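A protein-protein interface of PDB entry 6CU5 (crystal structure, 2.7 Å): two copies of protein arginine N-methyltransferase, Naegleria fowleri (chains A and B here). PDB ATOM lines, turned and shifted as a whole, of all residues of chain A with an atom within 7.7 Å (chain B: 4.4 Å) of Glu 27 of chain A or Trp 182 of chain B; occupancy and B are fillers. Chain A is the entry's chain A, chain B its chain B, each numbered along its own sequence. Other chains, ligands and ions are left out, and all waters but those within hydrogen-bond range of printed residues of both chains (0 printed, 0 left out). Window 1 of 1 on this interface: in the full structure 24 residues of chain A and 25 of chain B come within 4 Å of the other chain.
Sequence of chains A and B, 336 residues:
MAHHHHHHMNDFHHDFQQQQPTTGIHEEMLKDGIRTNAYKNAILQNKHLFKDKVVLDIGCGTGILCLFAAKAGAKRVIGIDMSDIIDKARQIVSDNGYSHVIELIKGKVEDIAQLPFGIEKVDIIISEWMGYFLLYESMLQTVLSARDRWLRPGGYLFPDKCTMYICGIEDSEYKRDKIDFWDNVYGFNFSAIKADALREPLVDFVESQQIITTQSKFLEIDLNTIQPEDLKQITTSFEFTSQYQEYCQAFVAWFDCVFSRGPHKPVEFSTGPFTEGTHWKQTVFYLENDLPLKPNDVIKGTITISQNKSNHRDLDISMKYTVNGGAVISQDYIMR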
ATOM      1  N   THR A  23      31.853 -10.562  23.242  1.00  0.00           N
ATOM      2  CA  THR A  23      31.266 -11.894  23.091  1.00  0.00           C
ATOM      3  C   THR A  23      31.675 -12.850  24.218  1.00  0.00           C
ATOM      4  O   THR A  23      30.875 -13.707  24.622  1.00  0.00           O
ATOM      5  CB  THR A  23      31.647 -12.483  21.742  1.00  0.00           C
ATOM      6  N   GLY A  24      32.925 -12.716  24.705  1.00  0.00           N
ATOM      7  CA  GLY A  24      33.345 -13.460  25.887  1.00  0.00           C
ATOM      8  C   GLY A  24      32.536 -13.090  27.116  1.00  0.00           C
ATOM      9  O   GLY A  24      32.334 -13.921  28.007  1.00  0.00           O
ATOM     10  N   ILE A  25      32.043 -11.850  27.166  1.00  0.00           N
ATOM     11  CA  ILE A  25      31.219 -11.403  28.288  1.00  0.00           C
ATOM     12  C   ILE A  25      29.906 -12.166  28.309  1.00  0.00           C
ATOM     13  O   ILE A  25      29.443 -12.619  29.361  1.00  0.00           O
ATOM     14  CB  ILE A  25      30.974  -9.886  28.210  1.00  0.00           C
ATOM     15  N   HIS A  26      29.266 -12.284  27.147  1.00  0.00           N
ATOM     16  CA  HIS A  26      27.924 -12.843  27.097  1.00  0.00           C
ATOM     17  C   HIS A  26      27.917 -14.353  27.308  1.00  0.00           C
ATOM     18  O   HIS A  26      26.974 -14.883  27.909  1.00  0.00           O
ATOM     19  CB  HIS A  26      27.276 -12.449  25.778  1.00  0.00           C
ATOM     20  CG  HIS A  26      27.300 -10.975  25.542  1.00  0.00           C
ATOM     21  ND1 HIS A  26      28.237 -10.363  24.735  1.00  0.00           N
ATOM     22  CD2 HIS A  26      26.541  -9.980  26.062  1.00  0.00           C
ATOM     23  CE1 HIS A  26      28.029  -9.058  24.737  1.00  0.00           C
ATOM     24  NE2 HIS A  26      27.009  -8.800  25.538  1.00  0.00           N
ATOM     25  N   GLU A  27      28.965 -15.063  26.894  1.00  0.00           N
ATOM     26  CA  GLU A  27      29.043 -16.467  27.276  1.00  0.00           C
ATOM     27  C   GLU A  27      29.123 -16.590  28.796  1.00  0.00           C
ATOM     28  O   GLU A  27      28.407 -17.393  29.408  1.00  0.00           O
ATOM     29  CB  GLU A  27      30.240 -17.156  26.603  1.00  0.00           C
ATOM     30  CG  GLU A  27      30.422 -18.605  27.089  1.00  0.00           C
ATOM     31  CD  GLU A  27      31.378 -19.457  26.243  1.00  0.00           C
ATOM     32  OE1 GLU A  27      31.979 -18.936  25.275  1.00  0.00           O
ATOM     33  OE2 GLU A  27      31.506 -20.667  26.541  1.00  0.00           O
ATOM     34  N   GLU A  28      29.978 -15.769  29.420  1.00  0.00           N
ATOM     35  CA  GLU A  28      30.108 -15.751  30.877  1.00  0.00           C
ATOM     36  C   GLU A  28      28.777 -15.421  31.544  1.00  0.00           C
ATOM     37  O   GLU A  28      28.343 -16.105  32.479  1.00  0.00           O
ATOM     38  CB  GLU A  28      31.176 -14.731  31.279  1.00  0.00           C
ATOM     39  CG  GLU A  28      31.378 -14.569  32.785  1.00  0.00           C
ATOM     40  CD  GLU A  28      32.639 -13.780  33.139  1.00  0.00           C
ATOM     41  OE1 GLU A  28      32.609 -12.527  33.088  1.00  0.00           O
ATOM     42  OE2 GLU A  28      33.661 -14.422  33.461  1.00  0.00           O
ATOM     43  N   MET A  29      28.104 -14.383  31.054  1.00  0.00           N
ATOM     44  CA  MET A  29      26.820 -13.992  31.614  1.00  0.00           C
ATOM     45  C   MET A  29      25.807 -15.136  31.516  1.00  0.00           C
ATOM     46  O   MET A  29      25.121 -15.459  32.498  1.00  0.00           O
ATOM     47  CB  MET A  29      26.320 -12.748  30.884  1.00  0.00           C
ATOM     48  CG  MET A  29      25.361 -11.857  31.641  1.00  0.00           C
ATOM     49  SD  MET A  29      26.211 -10.527  32.513  1.00  0.00           S
ATOM     50  CE  MET A  29      26.043 -11.101  34.176  1.00  0.00           C
ATOM     51  N   LEU A  30      25.699 -15.763  30.327  1.00  0.00           N
ATOM     52  CA  LEU A  30      24.664 -16.769  30.071  1.00  0.00           C
ATOM     53  C   LEU A  30      24.910 -18.077  30.809  1.00  0.00           C
ATOM     54  O   LEU A  30      23.947 -18.761  31.183  1.00  0.00           O
ATOM     55  CB  LEU A  30      24.557 -17.057  28.579  1.00  0.00           C
ATOM     56  CG  LEU A  30      23.896 -16.043  27.652  1.00  0.00           C
ATOM     57  CD1 LEU A  30      23.952 -16.560  26.200  1.00  0.00           C
ATOM     58  CD2 LEU A  30      22.455 -15.723  28.093  1.00  0.00           C
ATOM     59  N   LYS A  31      26.177 -18.458  30.999  1.00  0.00           N
ATOM     60  CA  LYS A  31      26.522 -19.623  31.803  1.00  0.00           C
ATOM     61  C   LYS A  31      26.367 -19.370  33.304  1.00  0.00           C
ATOM     62  O   LYS A  31      26.439 -20.330  34.077  1.00  0.00           O
ATOM     63  CB  LYS A  31      27.955 -20.055  31.486  1.00  0.00           C
ATOM     64  CG  LYS A  31      28.143 -20.684  30.114  1.00  0.00           C
ATOM     65  CD  LYS A  31      27.749 -22.159  30.118  1.00  0.00           C
ATOM     66  CE  LYS A  31      28.622 -22.994  29.181  1.00  0.00           C
ATOM     67  NZ  LYS A  31      29.236 -24.183  29.867  1.00  0.00           N
ATOM     68  N   ASP A  32      26.130 -18.120  33.728  1.00  0.00           N
ATOM     69  CA  ASP A  32      25.851 -17.795  35.131  1.00  0.00           C
ATOM     70  C   ASP A  32      24.402 -18.171  35.391  1.00  0.00           C
ATOM     71  O   ASP A  32      23.484 -17.384  35.148  1.00  0.00           O
ATOM     72  CB  ASP A  32      26.103 -16.320  35.428  1.00  0.00           C
ATOM     73  CG  ASP A  32      26.083 -15.997  36.936  1.00  0.00           C
ATOM     74  OD1 ASP A  32      25.767 -16.901  37.751  1.00  0.00           O
ATOM     75  OD2 ASP A  32      26.374 -14.833  37.292  1.00  0.00           O
ATOM     76  N   THR A  36      20.940 -15.885  35.682  1.00  0.00           N
ATOM     77  CA  THR A  36      20.004 -15.889  34.554  1.00  0.00           C
ATOM     78  C   THR A  36      18.650 -16.473  34.945  1.00  0.00           C
ATOM     79  O   THR A  36      17.605 -16.012  34.462  1.00  0.00           O
ATOM     80  CB  THR A  36      20.573 -16.662  33.352  1.00  0.00           C
ATOM     81  OG1 THR A  36      21.779 -16.054  32.885  1.00  0.00           O
ATOM     82  CG2 THR A  36      19.591 -16.636  32.206  1.00  0.00           C
ATOM     83  N   THR A  62      22.751 -10.502  23.823  1.00  0.00           N
ATOM     84  CA  THR A  62      22.214 -11.450  22.858  1.00  0.00           C
ATOM     85  C   THR A  62      20.699 -11.395  22.767  1.00  0.00           C
ATOM     86  O   THR A  62      20.137 -12.005  21.858  1.00  0.00           O
ATOM     87  CB  THR A  62      22.629 -12.879  23.213  1.00  0.00           C
ATOM     88  OG1 THR A  62      22.249 -13.176  24.568  1.00  0.00           O
ATOM     89  CG2 THR A  62      24.139 -13.097  23.015  1.00  0.00           C
ATOM     90  N   ILE A  85      27.358  -6.775  19.203  1.00  0.00           N
ATOM     91  CA  ILE A  85      26.670  -8.035  19.422  1.00  0.00           C
ATOM     92  C   ILE A  85      25.201  -7.937  19.062  1.00  0.00           C
ATOM     93  O   ILE A  85      24.548  -8.963  18.828  1.00  0.00           O
ATOM     94  CB  ILE A  85      26.819  -8.501  20.871  1.00  0.00           C
ATOM     95  CG1 ILE A  85      26.285  -9.927  20.956  1.00  0.00           C
ATOM     96  CG2 ILE A  85      26.011  -7.578  21.799  1.00  0.00           C
ATOM     97  CD1 ILE A  85      26.764 -10.735  22.098  1.00  0.00           C
ATOM     98  N   ILE A  92      19.223 -14.015  16.316  1.00  0.00           N
ATOM     99  CA  ILE A  92      18.664 -14.879  17.348  1.00  0.00           C
ATOM    100  C   ILE A  92      17.167 -14.620  17.516  1.00  0.00           C
ATOM    101  O   ILE A  92      16.383 -15.557  17.704  1.00  0.00           O
ATOM    102  CB  ILE A  92      19.449 -14.693  18.666  1.00  0.00           C
ATOM    103  CG1 ILE A  92      20.809 -15.397  18.569  1.00  0.00           C
ATOM    104  CG2 ILE A  92      18.673 -15.221  19.845  1.00  0.00           C
ATOM    105  CD1 ILE A  92      21.839 -14.921  19.557  1.00  0.00           C
ATOM    106  N   LYS B 178      30.979 -25.747  25.468  1.00  0.00           N
ATOM    107  CA  LYS B 178      31.341 -24.443  24.948  1.00  0.00           C
ATOM    108  C   LYS B 178      30.855 -24.236  23.529  1.00  0.00           C
ATOM    109  O   LYS B 178      30.656 -23.082  23.123  1.00  0.00           O
ATOM    110  CB  LYS B 178      32.867 -24.244  25.014  1.00  0.00           C
ATOM    111  N   ILE B 179      30.640 -25.338  22.792  1.00  0.00           N
ATOM    112  CA  ILE B 179      30.247 -25.339  21.386  1.00  0.00           C
ATOM    113  C   ILE B 179      28.771 -25.690  21.211  1.00  0.00           C
ATOM    114  O   ILE B 179      27.997 -24.888  20.676  1.00  0.00           O
ATOM    115  CB  ILE B 179      31.122 -26.329  20.590  1.00  0.00           C
ATOM    116  CG1 ILE B 179      32.599 -25.999  20.777  1.00  0.00           C
ATOM    117  CG2 ILE B 179      30.717 -26.356  19.106  1.00  0.00           C
ATOM    118  CD1 ILE B 179      32.991 -24.743  20.084  1.00  0.00           C
ATOM    119  N   ASP B 180      28.362 -26.875  21.673  1.00  0.00           N
ATOM    120  CA  ASP B 180      26.988 -27.319  21.450  1.00  0.00           C
ATOM    121  C   ASP B 180      25.988 -26.552  22.299  1.00  0.00           C
ATOM    122  O   ASP B 180      24.784 -26.586  22.011  1.00  0.00           O
ATOM    123  CB  ASP B 180      26.852 -28.819  21.759  1.00  0.00           C
ATOM    124  CG  ASP B 180      27.481 -29.710  20.695  1.00  0.00           C
ATOM    125  OD1 ASP B 180      27.592 -29.282  19.519  1.00  0.00           O
ATOM    126  OD2 ASP B 180      27.872 -30.841  21.055  1.00  0.00           O
ATOM    127  N   PHE B 181      26.484 -25.823  23.295  1.00  0.00           N
ATOM    128  CA  PHE B 181      25.644 -25.141  24.269  1.00  0.00           C
ATOM    129  C   PHE B 181      24.661 -24.173  23.610  1.00  0.00           C
ATOM    130  O   PHE B 181      23.503 -24.061  24.038  1.00  0.00           O
ATOM    131  CB  PHE B 181      26.564 -24.444  25.257  1.00  0.00           C
ATOM    132  CG  PHE B 181      25.951 -23.321  25.956  1.00  0.00           C
ATOM    133  CD1 PHE B 181      25.149 -23.543  27.054  1.00  0.00           C
ATOM    134  CD2 PHE B 181      26.167 -22.028  25.521  1.00  0.00           C
ATOM    135  CE1 PHE B 181      24.565 -22.502  27.712  1.00  0.00           C
ATOM    136  CE2 PHE B 181      25.583 -20.961  26.179  1.00  0.00           C
ATOM    137  CZ  PHE B 181      24.783 -21.199  27.280  1.00  0.00           C
ATOM    138  N   TRP B 182      25.081 -23.498  22.540  1.00  0.00           N
ATOM    139  CA  TRP B 182      24.249 -22.463  21.937  1.00  0.00           C
ATOM    140  C   TRP B 182      22.976 -22.993  21.251  1.00  0.00           C
ATOM    141  O   TRP B 182      22.087 -22.195  20.918  1.00  0.00           O
ATOM    142  CB  TRP B 182      25.114 -21.669  20.965  1.00  0.00           C
ATOM    143  CG  TRP B 182      26.338 -21.151  21.625  1.00  0.00           C
ATOM    144  CD1 TRP B 182      27.575 -21.713  21.610  1.00  0.00           C
ATOM    145  CD2 TRP B 182      26.439 -19.976  22.436  1.00  0.00           C
ATOM    146  NE1 TRP B 182      28.452 -20.951  22.351  1.00  0.00           N
ATOM    147  CE2 TRP B 182      27.778 -19.881  22.871  1.00  0.00           C
ATOM    148  CE3 TRP B 182      25.526 -18.995  22.836  1.00  0.00           C
ATOM    149  CZ2 TRP B 182      28.232 -18.843  23.672  1.00  0.00           C
ATOM    150  CZ3 TRP B 182      25.973 -17.969  23.632  1.00  0.00           C
ATOM    151  CH2 TRP B 182      27.320 -17.895  24.041  1.00  0.00           C
ATOM    152  N   ASP B 183      22.844 -24.308  21.062  1.00  0.00           N
ATOM    153  CA  ASP B 183      21.635 -24.849  20.455  1.00  0.00           C
ATOM    154  C   ASP B 183      20.426 -24.703  21.366  1.00  0.00           C
ATOM    155  O   ASP B 183      19.279 -24.694  20.887  1.00  0.00           O
ATOM    156  CB  ASP B 183      21.857 -26.305  20.077  1.00  0.00           C
ATOM    157  CG  ASP B 183      22.833 -26.445  18.949  1.00  0.00           C
ATOM    158  OD1 ASP B 183      22.828 -25.553  18.075  1.00  0.00           O
ATOM    159  OD2 ASP B 183      23.618 -27.424  18.944  1.00  0.00           O
ATOM    160  N   ASN B 184      20.657 -24.604  22.678  1.00  0.00           N
ATOM    161  CA  ASN B 184      19.562 -24.475  23.636  1.00  0.00           C
ATOM    162  C   ASN B 184      20.076 -23.660  24.823  1.00  0.00           C
ATOM    163  O   ASN B 184      20.704 -24.209  25.733  1.00  0.00           O
ATOM    164  CB  ASN B 184      19.085 -25.868  24.046  1.00  0.00           C
ATOM    165  CG  ASN B 184      17.975 -25.839  25.085  1.00  0.00           C
ATOM    166  OD1 ASN B 184      17.623 -24.791  25.613  1.00  0.00           O
ATOM    167  ND2 ASN B 184      17.410 -27.008  25.371  1.00  0.00           N
ATOM    168  N   VAL B 185      19.770 -22.362  24.821  1.00  0.00           N
ATOM    169  CA  VAL B 185      20.154 -21.430  25.875  1.00  0.00           C
ATOM    170  C   VAL B 185      18.876 -20.998  26.588  1.00  0.00           C
ATOM    171  O   VAL B 185      18.151 -20.128  26.093  1.00  0.00           O
ATOM    172  CB  VAL B 185      20.906 -20.219  25.310  1.00  0.00           C
ATOM    173  CG1 VAL B 185      21.413 -19.327  26.425  1.00  0.00           C
ATOM    174  CG2 VAL B 185      22.036 -20.660  24.452  1.00  0.00           C
ATOM    175  N   ASN B 189      16.905 -20.830  20.960  1.00  0.00           N
ATOM    176  CA  ASN B 189      17.806 -21.303  19.920  1.00  0.00           C
ATOM    177  C   ASN B 189      18.792 -20.184  19.621  1.00  0.00           C
ATOM    178  O   ASN B 189      18.426 -19.183  19.005  1.00  0.00           O
ATOM    179  CB  ASN B 189      16.997 -21.704  18.689  1.00  0.00           C
ATOM    180  CG  ASN B 189      17.833 -22.320  17.605  1.00  0.00           C
ATOM    181  OD1 ASN B 189      18.400 -21.621  16.769  1.00  0.00           O
ATOM    182  ND2 ASN B 189      17.899 -23.648  17.599  1.00  0.00           N
ATOM    183  N   PHE B 190      20.044 -20.366  20.054  1.00  0.00           N
ATOM    184  CA  PHE B 190      21.133 -19.406  19.877  1.00  0.00           C
ATOM    185  C   PHE B 190      22.190 -19.895  18.896  1.00  0.00           C
ATOM    186  O   PHE B 190      23.330 -19.427  18.945  1.00  0.00           O
ATOM    187  CB  PHE B 190      21.815 -19.103  21.212  1.00  0.00           C
ATOM    188  CG  PHE B 190      21.152 -18.022  22.023  1.00  0.00           C
ATOM    189  CD1 PHE B 190      19.842 -18.143  22.435  1.00  0.00           C
ATOM    190  CD2 PHE B 190      21.859 -16.901  22.403  1.00  0.00           C
ATOM    191  CE1 PHE B 190      19.245 -17.152  23.199  1.00  0.00           C
ATOM    192  CE2 PHE B 190      21.265 -15.917  23.170  1.00  0.00           C
ATOM    193  CZ  PHE B 190      19.958 -16.039  23.562  1.00  0.00           C
ATOM    194  N   SER B 191      21.847 -20.846  18.024  1.00  0.00           N
ATOM    195  CA  SER B 191      22.814 -21.419  17.093  1.00  0.00           C
ATOM    196  C   SER B 191      23.519 -20.385  16.225  1.00  0.00           C
ATOM    197  O   SER B 191      24.570 -20.691  15.665  1.00  0.00           O
ATOM    198  CB  SER B 191      22.116 -22.419  16.189  1.00  0.00           C
ATOM    199  OG  SER B 191      20.863 -21.900  15.799  1.00  0.00           O
ATOM    200  N   ILE B 193      25.327 -18.152  17.046  1.00  0.00           N
ATOM    201  CA  ILE B 193      26.649 -17.948  17.610  1.00  0.00           C
ATOM    202  C   ILE B 193      27.569 -19.138  17.361  1.00  0.00           C
ATOM    203  O   ILE B 193      28.794 -18.967  17.379  1.00  0.00           O
ATOM    204  CB  ILE B 193      26.487 -17.619  19.110  1.00  0.00           C
ATOM    205  CG1 ILE B 193      25.726 -16.293  19.259  1.00  0.00           C
ATOM    206  CG2 ILE B 193      27.832 -17.571  19.847  1.00  0.00           C
ATOM    207  CD1 ILE B 193      25.481 -15.852  20.706  1.00  0.00           C
ATOM    208  N   ALA B 197      31.807 -19.562  17.928  1.00  0.00           N
ATOM    209  CA  ALA B 197      32.367 -20.332  19.032  1.00  0.00           C
ATOM    210  C   ALA B 197      33.421 -21.319  18.529  1.00  0.00           C
ATOM    211  O   ALA B 197      34.469 -21.510  19.172  1.00  0.00           O
ATOM    212  CB  ALA B 197      31.255 -21.053  19.790  1.00  0.00           C
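The backbone carbonyl oxygen (O) of Lys 178 of chain B sits at hydrogen-bond distance from the indole nitrogen (NE1) of Trp 182 of chain B.
O of Trp 182 of chain B is in hydrogen-bond range of N of Phe 190 of chain B (2.9 Å).
The backbone NH of Ser 191 of chain B sits at hydrogen-bond distance from the backbone carbonyl oxygen of Trp 182 of chain B (3.2 Å).
CB of Glu 27 of chain A touches CZ2 of Trp 182 of chain B (3.9 Å).
CZ3 of Trp 182 of chain B touches CD1 of Leu 30 of chain A, at 3.6 Å.
CG1 of Val 185 of chain B touches CD1 of Leu 30 of chain A (3.8 Å).
Thr 62 of chain A touches Phe 190 of chain B (OG1 to CE2, 3.2 Å).
CG2 of Thr 62 of chain A touches CD1 of Ile 193 of chain B, 3.8 Å away.
CD1 of Ile 92 of chain A touches CD2 of Phe 190 of chain B, at 3.5 Å.
Ile 193 of chain B touches Ile 92 of chain A.
Of the printed residues of chain B, Glu 27 of chain A touches Trp 182 (3.9 Å).
Printed residues of chain A within 4 Å of Trp 182 of chain B: Glu 27 (3.9 Å) and Leu 30 (3.6 Å).
Printed residues of chain A within 4 Å of Phe 190 of chain B: Thr 62 and Ile 92.
Of the printed residues of chain A, Ile 193 of chain B touches Thr 62 and Ile 92.
Printed residues of chain B within 4 Å of Thr 62 of chain A: Phe 190 and Ile 193.
Of the printed residues of chain B, Leu 30 of chain A touches Trp 182 (3.6 Å) and Val 185 (3.8 Å).
The nearest residue of chain B that does not touch Glu 27 of chain A is Lys 178 of chain B (4.1 Å).
The nearest residue of chain A that does not touch Trp 182 of chain B is His 26 of chain A (4.9 Å).
Hydrophobic or aromatic side chains of chain A within 4 Å of the printed part of chain B: Leu 30 and Ile 92.
Among the printed residues, 7 pairs touch across the chains.
Among the printed residues, no Asp or Glu carboxylate lies within 4 Å of a Lys or Arg side-chain nitrogen of the other chain.
No position is printed for both chains.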
